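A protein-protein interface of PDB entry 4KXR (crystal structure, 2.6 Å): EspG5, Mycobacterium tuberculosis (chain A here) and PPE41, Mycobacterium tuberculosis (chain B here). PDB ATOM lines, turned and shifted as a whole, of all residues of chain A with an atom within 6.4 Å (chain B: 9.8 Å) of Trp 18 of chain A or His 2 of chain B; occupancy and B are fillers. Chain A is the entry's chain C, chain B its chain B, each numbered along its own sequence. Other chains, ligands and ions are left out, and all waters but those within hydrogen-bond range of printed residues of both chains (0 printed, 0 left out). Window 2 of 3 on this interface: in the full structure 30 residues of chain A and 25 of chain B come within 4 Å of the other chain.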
ATOM      1  N   VAL A  12      10.440 -28.348  17.668  1.00  0.00           N
ATOM      2  CA  VAL A  12      10.927 -27.110  18.220  1.00  0.00           C
ATOM      3  C   VAL A  12      12.061 -26.607  17.322  1.00  0.00           C
ATOM      4  O   VAL A  12      12.672 -27.397  16.594  1.00  0.00           O
ATOM      5  CB  VAL A  12      11.380 -27.340  19.692  1.00  0.00           C
ATOM      6  CG1 VAL A  12      12.762 -27.980  19.781  1.00  0.00           C
ATOM      7  CG2 VAL A  12      11.372 -26.041  20.462  1.00  0.00           C
ATOM      8  N   ASN A  13      12.331 -25.305  17.344  1.00  0.00           N
ATOM      9  CA  ASN A  13      13.527 -24.793  16.694  1.00  0.00           C
ATOM     10  C   ASN A  13      14.729 -24.798  17.649  1.00  0.00           C
ATOM     11  O   ASN A  13      14.645 -25.285  18.785  1.00  0.00           O
ATOM     12  CB  ASN A  13      13.270 -23.419  16.064  1.00  0.00           C
ATOM     13  CG  ASN A  13      13.476 -22.260  17.023  1.00  0.00           C
ATOM     14  OD1 ASN A  13      13.706 -22.436  18.218  1.00  0.00           O
ATOM     15  ND2 ASN A  13      13.395 -21.056  16.489  1.00  0.00           N
ATOM     16  N   VAL A  14      15.851 -24.257  17.192  1.00  0.00           N
ATOM     17  CA  VAL A  14      17.104 -24.358  17.948  1.00  0.00           C
ATOM     18  C   VAL A  14      17.062 -23.584  19.272  1.00  0.00           C
ATOM     19  O   VAL A  14      17.650 -24.023  20.260  1.00  0.00           O
ATOM     20  CB  VAL A  14      18.301 -23.879  17.101  1.00  0.00           C
ATOM     21  CG1 VAL A  14      19.609 -24.008  17.881  1.00  0.00           C
ATOM     22  CG2 VAL A  14      18.355 -24.673  15.805  1.00  0.00           C
ATOM     23  N   ASP A  15      16.378 -22.433  19.274  1.00  0.00           N
ATOM     24  CA  ASP A  15      16.196 -21.633  20.493  1.00  0.00           C
ATOM     25  C   ASP A  15      15.198 -22.294  21.448  1.00  0.00           C
ATOM     26  O   ASP A  15      15.468 -22.410  22.635  1.00  0.00           O
ATOM     27  CB  ASP A  15      15.773 -20.194  20.164  1.00  0.00           C
ATOM     28  CG  ASP A  15      16.962 -19.266  19.961  1.00  0.00           C
ATOM     29  OD1 ASP A  15      18.077 -19.613  20.405  1.00  0.00           O
ATOM     30  OD2 ASP A  15      16.781 -18.183  19.370  1.00  0.00           O
ATOM     31  N   GLY A  16      14.067 -22.747  20.923  1.00  0.00           N
ATOM     32  CA  GLY A  16      13.123 -23.502  21.714  1.00  0.00           C
ATOM     33  C   GLY A  16      13.756 -24.737  22.335  1.00  0.00           C
ATOM     34  O   GLY A  16      13.475 -25.081  23.477  1.00  0.00           O
ATOM     35  N   PHE A  17      14.621 -25.402  21.586  1.00  0.00           N
ATOM     36  CA  PHE A  17      15.370 -26.525  22.130  1.00  0.00           C
ATOM     37  C   PHE A  17      16.288 -26.100  23.288  1.00  0.00           C
ATOM     38  O   PHE A  17      16.481 -26.865  24.235  1.00  0.00           O
ATOM     39  CB  PHE A  17      16.206 -27.199  21.036  1.00  0.00           C
ATOM     40  CG  PHE A  17      16.610 -28.601  21.368  1.00  0.00           C
ATOM     41  CD1 PHE A  17      17.786 -28.856  22.049  1.00  0.00           C
ATOM     42  CD2 PHE A  17      15.793 -29.670  21.017  1.00  0.00           C
ATOM     43  CE1 PHE A  17      18.154 -30.156  22.364  1.00  0.00           C
ATOM     44  CE2 PHE A  17      16.153 -30.971  21.318  1.00  0.00           C
ATOM     45  CZ  PHE A  17      17.339 -31.219  21.993  1.00  0.00           C
ATOM     46  N   TRP A  18      16.861 -24.900  23.202  1.00  0.00           N
ATOM     47  CA  TRP A  18      17.731 -24.393  24.262  1.00  0.00           C
ATOM     48  C   TRP A  18      16.968 -24.109  25.534  1.00  0.00           C
ATOM     49  O   TRP A  18      17.510 -24.286  26.619  1.00  0.00           O
ATOM     50  CB  TRP A  18      18.454 -23.122  23.845  1.00  0.00           C
ATOM     51  CG  TRP A  18      19.593 -22.785  24.765  1.00  0.00           C
ATOM     52  CD1 TRP A  18      20.839 -23.356  24.784  1.00  0.00           C
ATOM     53  CD2 TRP A  18      19.591 -21.804  25.799  1.00  0.00           C
ATOM     54  NE1 TRP A  18      21.610 -22.788  25.762  1.00  0.00           N
ATOM     55  CE2 TRP A  18      20.868 -21.831  26.404  1.00  0.00           C
ATOM     56  CE3 TRP A  18      18.629 -20.907  26.281  1.00  0.00           C
ATOM     57  CZ2 TRP A  18      21.214 -20.985  27.461  1.00  0.00           C
ATOM     58  CZ3 TRP A  18      18.972 -20.070  27.331  1.00  0.00           C
ATOM     59  CH2 TRP A  18      20.258 -20.111  27.907  1.00  0.00           C
ATOM     60  N   MET A  19      15.724 -23.656  25.408  1.00  0.00           N
ATOM     61  CA  MET A  19      14.871 -23.456  26.569  1.00  0.00           C
ATOM     62  C   MET A  19      14.569 -24.751  27.305  1.00  0.00           C
ATOM     63  O   MET A  19      14.580 -24.783  28.547  1.00  0.00           O
ATOM     64  CB  MET A  19      13.558 -22.830  26.160  1.00  0.00           C
ATOM     65  CG  MET A  19      13.690 -21.388  25.763  1.00  0.00           C
ATOM     66  SD  MET A  19      12.035 -20.743  25.513  1.00  0.00           S
ATOM     67  CE  MET A  19      12.322 -19.887  23.945  1.00  0.00           C
ATOM     68  N   LEU A  20      14.278 -25.809  26.554  1.00  0.00           N
ATOM     69  CA  LEU A  20      14.069 -27.113  27.168  1.00  0.00           C
ATOM     70  C   LEU A  20      15.319 -27.533  27.940  1.00  0.00           C
ATOM     71  O   LEU A  20      15.221 -28.066  29.043  1.00  0.00           O
ATOM     72  CB  LEU A  20      13.693 -28.162  26.129  1.00  0.00           C
ATOM     73  CG  LEU A  20      12.393 -27.904  25.358  1.00  0.00           C
ATOM     74  CD1 LEU A  20      12.138 -29.019  24.345  1.00  0.00           C
ATOM     75  CD2 LEU A  20      11.208 -27.759  26.298  1.00  0.00           C
ATOM     76  N   GLN A  21      16.487 -27.248  27.377  1.00  0.00           N
ATOM     77  CA  GLN A  21      17.753 -27.519  28.047  1.00  0.00           C
ATOM     78  C   GLN A  21      17.864 -26.779  29.384  1.00  0.00           C
ATOM     79  O   GLN A  21      18.274 -27.357  30.383  1.00  0.00           O
ATOM     80  CB  GLN A  21      18.932 -27.122  27.149  1.00  0.00           C
ATOM     81  CG  GLN A  21      19.094 -27.970  25.895  1.00  0.00           C
ATOM     82  CD  GLN A  21      20.337 -27.606  25.118  1.00  0.00           C
ATOM     83  OE1 GLN A  21      20.274 -26.897  24.110  1.00  0.00           O
ATOM     84  NE2 GLN A  21      21.484 -28.070  25.598  1.00  0.00           N
ATOM     85  N   ALA A  22      17.516 -25.495  29.372  1.00  0.00           N
ATOM     86  CA  ALA A  22      17.484 -24.665  30.579  1.00  0.00           C
ATOM     87  C   ALA A  22      16.427 -25.161  31.574  1.00  0.00           C
ATOM     88  O   ALA A  22      16.691 -25.243  32.779  1.00  0.00           O
ATOM     89  CB  ALA A  22      17.222 -23.197  30.221  1.00  0.00           C
ATOM     90  N   LEU A  23      15.234 -25.478  31.072  1.00  0.00           N
ATOM     91  CA  LEU A  23      14.151 -25.919  31.943  1.00  0.00           C
ATOM     92  C   LEU A  23      14.465 -27.250  32.626  1.00  0.00           C
ATOM     93  O   LEU A  23      13.987 -27.488  33.730  1.00  0.00           O
ATOM     94  CB  LEU A  23      12.840 -26.043  31.165  1.00  0.00           C
ATOM     95  CG  LEU A  23      12.142 -24.744  30.782  1.00  0.00           C
ATOM     96  CD1 LEU A  23      11.072 -25.014  29.740  1.00  0.00           C
ATOM     97  CD2 LEU A  23      11.531 -24.072  31.995  1.00  0.00           C
ATOM     98  N   ILE A  26      19.991 -29.598  31.228  1.00  0.00           N
ATOM     99  CA  ILE A  26      20.733 -30.501  30.356  1.00  0.00           C
ATOM    100  C   ILE A  26      21.786 -29.678  29.650  1.00  0.00           C
ATOM    101  O   ILE A  26      21.456 -28.670  29.022  1.00  0.00           O
ATOM    102  CB  ILE A  26      19.833 -31.112  29.255  1.00  0.00           C
ATOM    103  CG1 ILE A  26      18.627 -31.848  29.861  1.00  0.00           C
ATOM    104  CG2 ILE A  26      20.646 -32.054  28.372  1.00  0.00           C
ATOM    105  CD1 ILE A  26      17.553 -32.230  28.859  1.00  0.00           C
ATOM    106  N   CYS A  35      22.920 -27.882  18.486  1.00  0.00           N
ATOM    107  CA  CYS A  35      22.387 -26.940  19.449  1.00  0.00           C
ATOM    108  C   CYS A  35      23.487 -26.199  20.241  1.00  0.00           C
ATOM    109  O   CYS A  35      24.669 -26.461  20.076  1.00  0.00           O
ATOM    110  CB  CYS A  35      21.451 -27.697  20.377  1.00  0.00           C
ATOM    111  SG  CYS A  35      20.059 -28.329  19.420  1.00  0.00           S
ATOM    112  N   ARG A  36      23.087 -25.245  21.078  1.00  0.00           N
ATOM    113  CA  ARG A  36      24.044 -24.494  21.900  1.00  0.00           C
ATOM    114  C   ARG A  36      24.141 -25.215  23.224  1.00  0.00           C
ATOM    115  O   ARG A  36      23.148 -25.763  23.689  1.00  0.00           O
ATOM    116  CB  ARG A  36      23.599 -23.026  22.101  1.00  0.00           C
ATOM    117  CG  ARG A  36      23.880 -22.131  20.893  1.00  0.00           C
ATOM    118  CD  ARG A  36      23.482 -20.657  21.083  1.00  0.00           C
ATOM    119  NE  ARG A  36      22.028 -20.438  21.175  1.00  0.00           N
ATOM    120  CZ  ARG A  36      21.353 -20.118  22.289  1.00  0.00           C
ATOM    121  NH1 ARG A  36      21.971 -19.952  23.462  1.00  0.00           N
ATOM    122  NH2 ARG A  36      20.033 -19.955  22.239  1.00  0.00           N
ATOM    123  N   PRO A  37      25.342 -25.239  23.831  1.00  0.00           N
ATOM    124  CA  PRO A  37      25.393 -25.764  25.196  1.00  0.00           C
ATOM    125  C   PRO A  37      24.633 -24.853  26.162  1.00  0.00           C
ATOM    126  O   PRO A  37      24.391 -23.672  25.844  1.00  0.00           O
ATOM    127  CB  PRO A  37      26.897 -25.809  25.519  1.00  0.00           C
ATOM    128  CG  PRO A  37      27.546 -24.920  24.522  1.00  0.00           C
ATOM    129  CD  PRO A  37      26.683 -24.934  23.300  1.00  0.00           C
ATOM    130  N   TYR A  38      24.235 -25.416  27.302  1.00  0.00           N
ATOM    131  CA  TYR A  38      23.600 -24.660  28.374  1.00  0.00           C
ATOM    132  C   TYR A  38      24.488 -24.708  29.607  1.00  0.00           C
ATOM    133  O   TYR A  38      24.887 -25.787  30.025  1.00  0.00           O
ATOM    134  CB  TYR A  38      22.232 -25.244  28.687  1.00  0.00           C
ATOM    135  CG  TYR A  38      21.616 -24.709  29.950  1.00  0.00           C
ATOM    136  CD1 TYR A  38      21.114 -23.409  30.011  1.00  0.00           C
ATOM    137  CD2 TYR A  38      21.521 -25.505  31.096  1.00  0.00           C
ATOM    138  CE1 TYR A  38      20.536 -22.917  31.182  1.00  0.00           C
ATOM    139  CE2 TYR A  38      20.945 -25.023  32.265  1.00  0.00           C
ATOM    140  CZ  TYR A  38      20.457 -23.731  32.306  1.00  0.00           C
ATOM    141  OH  TYR A  38      19.879 -23.264  33.465  1.00  0.00           O
ATOM    142  N   VAL A  39      24.787 -23.540  30.186  1.00  0.00           N
ATOM    143  CA  VAL A  39      25.749 -23.425  31.306  1.00  0.00           C
ATOM    144  C   VAL A  39      25.093 -23.004  32.642  1.00  0.00           C
ATOM    145  O   VAL A  39      24.182 -22.181  32.691  1.00  0.00           O
ATOM    146  CB  VAL A  39      26.929 -22.491  30.908  1.00  0.00           C
ATOM    147  CG1 VAL A  39      27.848 -22.213  32.083  1.00  0.00           C
ATOM    148  CG2 VAL A  39      27.724 -23.097  29.761  1.00  0.00           C
ATOM    149  N   MET B   1      23.893 -12.158  31.821  1.00  0.00           N
ATOM    150  CA  MET B   1      24.658 -12.343  30.551  1.00  0.00           C
ATOM    151  C   MET B   1      24.987 -13.842  30.411  1.00  0.00           C
ATOM    152  O   MET B   1      25.560 -14.442  31.324  1.00  0.00           O
ATOM    153  CB  MET B   1      25.948 -11.483  30.542  1.00  0.00           C
ATOM    154  CG  MET B   1      25.831 -10.071  31.166  1.00  0.00           C
ATOM    155  SD  MET B   1      27.386  -9.238  31.651  1.00  0.00           S
ATOM    156  CE  MET B   1      26.860  -8.349  33.122  1.00  0.00           C
ATOM    157  N   HIS B   2      24.588 -14.443  29.288  1.00  0.00           N
ATOM    158  CA  HIS B   2      24.917 -15.839  28.958  1.00  0.00           C
ATOM    159  C   HIS B   2      25.930 -15.853  27.814  1.00  0.00           C
ATOM    160  O   HIS B   2      25.550 -15.798  26.634  1.00  0.00           O
ATOM    161  CB  HIS B   2      23.669 -16.616  28.519  1.00  0.00           C
ATOM    162  CG  HIS B   2      22.702 -16.896  29.627  1.00  0.00           C
ATOM    163  ND1 HIS B   2      22.481 -18.168  30.118  1.00  0.00           N
ATOM    164  CD2 HIS B   2      21.890 -16.070  30.334  1.00  0.00           C
ATOM    165  CE1 HIS B   2      21.576 -18.112  31.082  1.00  0.00           C
ATOM    166  NE2 HIS B   2      21.203 -16.851  31.232  1.00  0.00           N
ATOM    167  N   PHE B   3      27.211 -15.934  28.157  1.00  0.00           N
ATOM    168  CA  PHE B   3      28.244 -15.934  27.140  1.00  0.00           C
ATOM    169  C   PHE B   3      28.294 -17.244  26.338  1.00  0.00           C
ATOM    170  O   PHE B   3      28.919 -17.279  25.289  1.00  0.00           O
ATOM    171  CB  PHE B   3      29.591 -15.561  27.742  1.00  0.00           C
ATOM    172  CG  PHE B   3      29.596 -14.203  28.384  1.00  0.00           C
ATOM    173  CD1 PHE B   3      29.782 -13.056  27.619  1.00  0.00           C
ATOM    174  CD2 PHE B   3      29.376 -14.059  29.747  1.00  0.00           C
ATOM    175  CE1 PHE B   3      29.759 -11.797  28.202  1.00  0.00           C
ATOM    176  CE2 PHE B   3      29.367 -12.795  30.339  1.00  0.00           C
ATOM    177  CZ  PHE B   3      29.553 -11.666  29.561  1.00  0.00           C
ATOM    178  N   GLU B   4      27.588 -18.288  26.788  1.00  0.00           N
ATOM    179  CA  GLU B   4      27.383 -19.480  25.960  1.00  0.00           C
ATOM    180  C   GLU B   4      26.509 -19.210  24.737  1.00  0.00           C
ATOM    181  O   GLU B   4      26.436 -20.042  23.830  1.00  0.00           O
ATOM    182  CB  GLU B   4      26.806 -20.634  26.761  1.00  0.00           C
ATOM    183  CG  GLU B   4      25.390 -20.429  27.320  1.00  0.00           C
ATOM    184  CD  GLU B   4      25.364 -19.898  28.743  1.00  0.00           C
ATOM    185  OE1 GLU B   4      26.022 -18.861  29.015  1.00  0.00           O
ATOM    186  OE2 GLU B   4      24.668 -20.521  29.586  1.00  0.00           O
ATOM    187  N   ALA B   5      25.849 -18.049  24.697  1.00  0.00           N
ATOM    188  CA  ALA B   5      25.237 -17.547  23.455  1.00  0.00           C
ATOM    189  C   ALA B   5      26.243 -17.433  22.320  1.00  0.00           C
ATOM    190  O   ALA B   5      25.854 -17.506  21.162  1.00  0.00           O
ATOM    191  CB  ALA B   5      24.613 -16.190  23.678  1.00  0.00           C
ATOM    192  N   TYR B   6      27.519 -17.258  22.658  1.00  0.00           N
ATOM    193  CA  TYR B   6      28.561 -17.004  21.677  1.00  0.00           C
ATOM    194  C   TYR B   6      29.557 -18.156  21.575  1.00  0.00           C
ATOM    195  O   TYR B   6      29.864 -18.819  22.584  1.00  0.00           O
ATOM    196  CB  TYR B   6      29.309 -15.713  22.043  1.00  0.00           C
ATOM    197  CG  TYR B   6      28.389 -14.539  22.344  1.00  0.00           C
ATOM    198  CD1 TYR B   6      27.299 -14.247  21.530  1.00  0.00           C
ATOM    199  CD2 TYR B   6      28.626 -13.713  23.443  1.00  0.00           C
ATOM    200  CE1 TYR B   6      26.468 -13.165  21.816  1.00  0.00           C
ATOM    201  CE2 TYR B   6      27.809 -12.638  23.732  1.00  0.00           C
ATOM    202  CZ  TYR B   6      26.740 -12.356  22.922  1.00  0.00           C
ATOM    203  OH  TYR B   6      25.942 -11.289  23.237  1.00  0.00           O
ATOM    204  N   PRO B   7      30.089 -18.386  20.364  1.00  0.00           N
ATOM    205  CA  PRO B   7      31.074 -19.457  20.124  1.00  0.00           C
ATOM    206  C   PRO B   7      32.397 -19.183  20.816  1.00  0.00           C
ATOM    207  O   PRO B   7      32.679 -18.059  21.141  1.00  0.00           O
ATOM    208  CB  PRO B   7      31.305 -19.391  18.602  1.00  0.00           C
ATOM    209  CG  PRO B   7      30.984 -17.968  18.246  1.00  0.00           C
ATOM    210  CD  PRO B   7      29.859 -17.565  19.159  1.00  0.00           C
ATOM    211  N   VAL B  10      34.823 -16.311  19.844  1.00  0.00           N
ATOM    212  CA  VAL B  10      34.447 -15.006  20.376  1.00  0.00           C
ATOM    213  C   VAL B  10      34.901 -14.812  21.822  1.00  0.00           C
ATOM    214  O   VAL B  10      35.569 -13.827  22.142  1.00  0.00           O
ATOM    215  CB  VAL B  10      32.923 -14.825  20.325  1.00  0.00           C
ATOM    216  CG1 VAL B  10      32.482 -13.574  21.063  1.00  0.00           C
ATOM    217  CG2 VAL B  10      32.478 -14.740  18.881  1.00  0.00           C
ATOM    218  N   ASN B  11      34.518 -15.738  22.699  1.00  0.00           N
ATOM    219  CA  ASN B  11      34.896 -15.649  24.105  1.00  0.00           C
ATOM    220  C   ASN B  11      36.427 -15.721  24.316  1.00  0.00           C
ATOM    221  O   ASN B  11      36.985 -14.946  25.104  1.00  0.00           O
ATOM    222  CB  ASN B  11      34.173 -16.715  24.933  1.00  0.00           C
ATOM    223  CG  ASN B  11      32.674 -16.453  25.074  1.00  0.00           C
ATOM    224  OD1 ASN B  11      32.254 -15.315  25.277  1.00  0.00           O
ATOM    225  ND2 ASN B  11      31.866 -17.510  24.985  1.00  0.00           N
ATOM    226  N   TRP B 143      33.242 -24.490  23.613  1.00  0.00           N
ATOM    227  CA  TRP B 143      32.139 -23.515  23.740  1.00  0.00           C
ATOM    228  C   TRP B 143      31.638 -23.513  25.177  1.00  0.00           C
ATOM    229  O   TRP B 143      31.524 -22.465  25.814  1.00  0.00           O
ATOM    230  CB  TRP B 143      31.014 -23.932  22.785  1.00  0.00           C
ATOM    231  CG  TRP B 143      29.945 -22.972  22.490  1.00  0.00           C
ATOM    232  CD1 TRP B 143      29.268 -22.214  23.362  1.00  0.00           C
ATOM    233  CD2 TRP B 143      29.331 -22.769  21.218  1.00  0.00           C
ATOM    234  NE1 TRP B 143      28.280 -21.500  22.716  1.00  0.00           N
ATOM    235  CE2 TRP B 143      28.313 -21.815  21.392  1.00  0.00           C
ATOM    236  CE3 TRP B 143      29.557 -23.294  19.935  1.00  0.00           C
ATOM    237  CZ2 TRP B 143      27.533 -21.352  20.343  1.00  0.00           C
ATOM    238  CZ3 TRP B 143      28.774 -22.845  18.892  1.00  0.00           C
ATOM    239  CH2 TRP B 143      27.766 -21.881  19.105  1.00  0.00           C
ATOM    240  N   ASP B 144      31.339 -24.709  25.671  1.00  0.00           N
ATOM    241  CA  ASP B 144      30.944 -24.920  27.067  1.00  0.00           C
ATOM    242  C   ASP B 144      31.968 -24.383  28.058  1.00  0.00           C
ATOM    243  O   ASP B 144      31.598 -23.683  28.964  1.00  0.00           O
ATOM    244  CB  ASP B 144      30.732 -26.415  27.339  1.00  0.00           C
ATOM    245  CG  ASP B 144      30.286 -26.690  28.753  1.00  0.00           C
ATOM    246  OD1 ASP B 144      31.103 -26.696  29.709  1.00  0.00           O
ATOM    247  OD2 ASP B 144      29.081 -26.893  28.916  1.00  0.00           O
ATOM    248  N   ASP B 146      34.454 -22.127  27.770  1.00  0.00           N
ATOM    249  CA  ASP B 146      34.507 -20.675  27.733  1.00  0.00           C
ATOM    250  C   ASP B 146      33.258 -20.038  28.373  1.00  0.00           C
ATOM    251  O   ASP B 146      33.307 -18.966  28.992  1.00  0.00           O
ATOM    252  CB  ASP B 146      34.606 -20.190  26.286  1.00  0.00           C
ATOM    253  CG  ASP B 146      36.015 -20.286  25.706  1.00  0.00           C
ATOM    254  OD1 ASP B 146      36.915 -20.919  26.321  1.00  0.00           O
ATOM    255  OD2 ASP B 146      36.184 -19.702  24.608  1.00  0.00           O
ATOM    256  N   GLY B 147      32.134 -20.704  28.200  1.00  0.00           N
ATOM    257  CA  GLY B 147      30.893 -20.252  28.771  1.00  0.00           C
ATOM    258  C   GLY B 147      30.996 -20.226  30.272  1.00  0.00           C
ATOM    259  O   GLY B 147      30.625 -19.232  30.909  1.00  0.00           O
ATOM    260  N   GLU B 148      31.521 -21.298  30.849  1.00  0.00           N
ATOM    261  CA  GLU B 148      31.606 -21.315  32.297  1.00  0.00           C
ATOM    262  C   GLU B 148      32.747 -20.486  32.842  1.00  0.00           C
ATOM    263  O   GLU B 148      32.647 -19.990  33.952  1.00  0.00           O
ATOM    264  CB  GLU B 148      31.522 -22.699  32.935  1.00  0.00           C
ATOM    265  CG  GLU B 148      32.215 -23.846  32.277  1.00  0.00           C
ATOM    266  CD  GLU B 148      32.009 -25.138  33.069  1.00  0.00           C
ATOM    267  OE1 GLU B 148      30.834 -25.491  33.322  1.00  0.00           O
ATOM    268  OE2 GLU B 148      33.020 -25.789  33.441  1.00  0.00           O
ATOM    269  N   MET B 150      33.607 -17.532  31.490  1.00  0.00           N
ATOM    270  CA  MET B 150      32.962 -16.222  31.527  1.00  0.00           C
ATOM    271  C   MET B 150      31.864 -16.087  32.603  1.00  0.00           C
ATOM    272  O   MET B 150      31.714 -15.024  33.196  1.00  0.00           O
ATOM    273  CB  MET B 150      32.405 -15.892  30.165  1.00  0.00           C
ATOM    274  CG  MET B 150      33.479 -15.593  29.127  1.00  0.00           C
ATOM    275  SD  MET B 150      34.461 -14.132  29.528  1.00  0.00           S
ATOM    276  CE  MET B 150      33.187 -12.899  29.752  1.00  0.00           C
ATOM    277  N   ARG B 151      31.114 -17.148  32.893  1.00  0.00           N
ATOM    278  CA  ARG B 151      30.182 -17.084  34.007  1.00  0.00           C
ATOM    279  C   ARG B 151      30.906 -16.774  35.314  1.00  0.00           C
ATOM    280  O   ARG B 151      30.460 -15.913  36.062  1.00  0.00           O
ATOM    281  CB  ARG B 151      29.402 -18.386  34.167  1.00  0.00           C
ATOM    282  CG  ARG B 151      28.340 -18.352  35.277  1.00  0.00           C
ATOM    283  CD  ARG B 151      27.913 -19.764  35.672  1.00  0.00           C
ATOM    284  NE  ARG B 151      29.093 -20.540  36.058  1.00  0.00           N
ATOM    285  CZ  ARG B 151      29.273 -21.849  35.874  1.00  0.00           C
ATOM    286  NH1 ARG B 151      28.338 -22.600  35.294  1.00  0.00           N
ATOM    287  NH2 ARG B 151      30.426 -22.399  36.261  1.00  0.00           N
ATOM    288  N   ARG B 154      32.206 -13.191  35.414  1.00  0.00           N
ATOM    289  CA  ARG B 154      31.114 -12.260  35.682  1.00  0.00           C
ATOM    290  C   ARG B 154      30.770 -12.228  37.149  1.00  0.00           C
ATOM    291  O   ARG B 154      30.600 -11.167  37.710  1.00  0.00           O
ATOM    292  CB  ARG B 154      29.864 -12.632  34.871  1.00  0.00           C
ATOM    293  CG  ARG B 154      28.686 -11.709  35.105  1.00  0.00           C
ATOM    294  CD  ARG B 154      27.450 -12.117  34.327  1.00  0.00           C
ATOM    295  NE  ARG B 154      27.042 -13.520  34.491  1.00  0.00           N
ATOM    296  CZ  ARG B 154      26.358 -14.021  35.525  1.00  0.00           C
ATOM    297  NH1 ARG B 154      26.005 -13.268  36.566  1.00  0.00           N
ATOM    298  NH2 ARG B 154      26.040 -15.306  35.520  1.00  0.00           N
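OE2 of Glu 4 of chain B lies within hydrogen-bond range of N of Val 39 of chain A, 3.1 Å away.
The side-chain amide oxygen (OE1) of Gln 21 of chain A lies close to the backbone carbonyl oxygen (O) of Arg 36 of chain A. The backbone carbonyl oxygen (O) of Glu 4 of chain B lies within hydrogen-bond range of the indole nitrogen (NE1) of Trp 143 of chain B (2.6 Å). NE1 of Trp 18 of chain A is in hydrogen-bond range of O of Pro 37 of chain A, 2.9 Å away. The indole nitrogen of Trp 143 of chain B lies within hydrogen-bond range of the backbone carbonyl oxygen of Tyr 6 of chain B (3.1 Å). The side-chain carboxylate (OE2) of Glu 4 of chain B sits at hydrogen-bond distance from a ring nitrogen (ND1) of His 2 of chain B (3.3 Å). OD1 of Asp 15 of chain A lies within salt-bridge range of NH2 of Arg 36 of chain A (2.7 Å).
Among the printed residues, pairs that only touch across the chains: Val 39 of chain A with Arg 151 of chain B, Pro 37 of chain A with Trp 143 of chain B, Trp 18 of chain A with His 2 of chain B, Pro 37 of chain A with Glu 4 of chain B, Arg 36 of chain A with Trp 143 of chain B, Val 39 of chain A with Glu 148 of chain B, Arg 36 of chain A with Ala 5 of chain B, Pro 37 of chain A with Asp 144 of chain B and Val 39 of chain A with Asp 144 of chain B.
No residue of chain B comes within 4 Å of Gln 21 of chain A. Of chain B, only Ala 5 and Trp 143 come within 4 Å of Arg 36 of chain A. Printed residues of chain B within 4 Å of Pro 37 of chain A: Glu 4 (3.7 Å), Trp 143 (3.4 Å) and Asp 144 (3.97 Å). Of the printed residues of chain B, Val 39 of chain A touches Glu 4 (3.1 Å), Asp 144 (3.998 Å), Glu 148 (3.8 Å) and Arg 151 (3.3 Å). His 2 of chain B touches one residue of chain A. Pro 7 of chain B touches none of the printed residues of chain A. Printed residues of chain A within 4 Å of Trp 143 of chain B: Arg 36 and Pro 37. The nearest residue of chain B that does not touch Trp 18 of chain A is Glu 4 of chain B (4.1 Å). The nearest printed residue of chain A that does not touch Asp 144 of chain B is Tyr 38 of chain A (4.5 Å).
Of the 18 printed residues of chain A, 4 touch a printed residue of chain B. Hydrophobic or aromatic side chains of chain A that line the printed part of chain B: Trp 18, Pro 37 and Val 39. Of the 17 printed residues of chain B, 7 touch a printed residue of chain A. Among the printed residues, no Asp or Glu carboxylate lies within 4 Å of a Lys or Arg side-chain nitrogen of the other chain.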
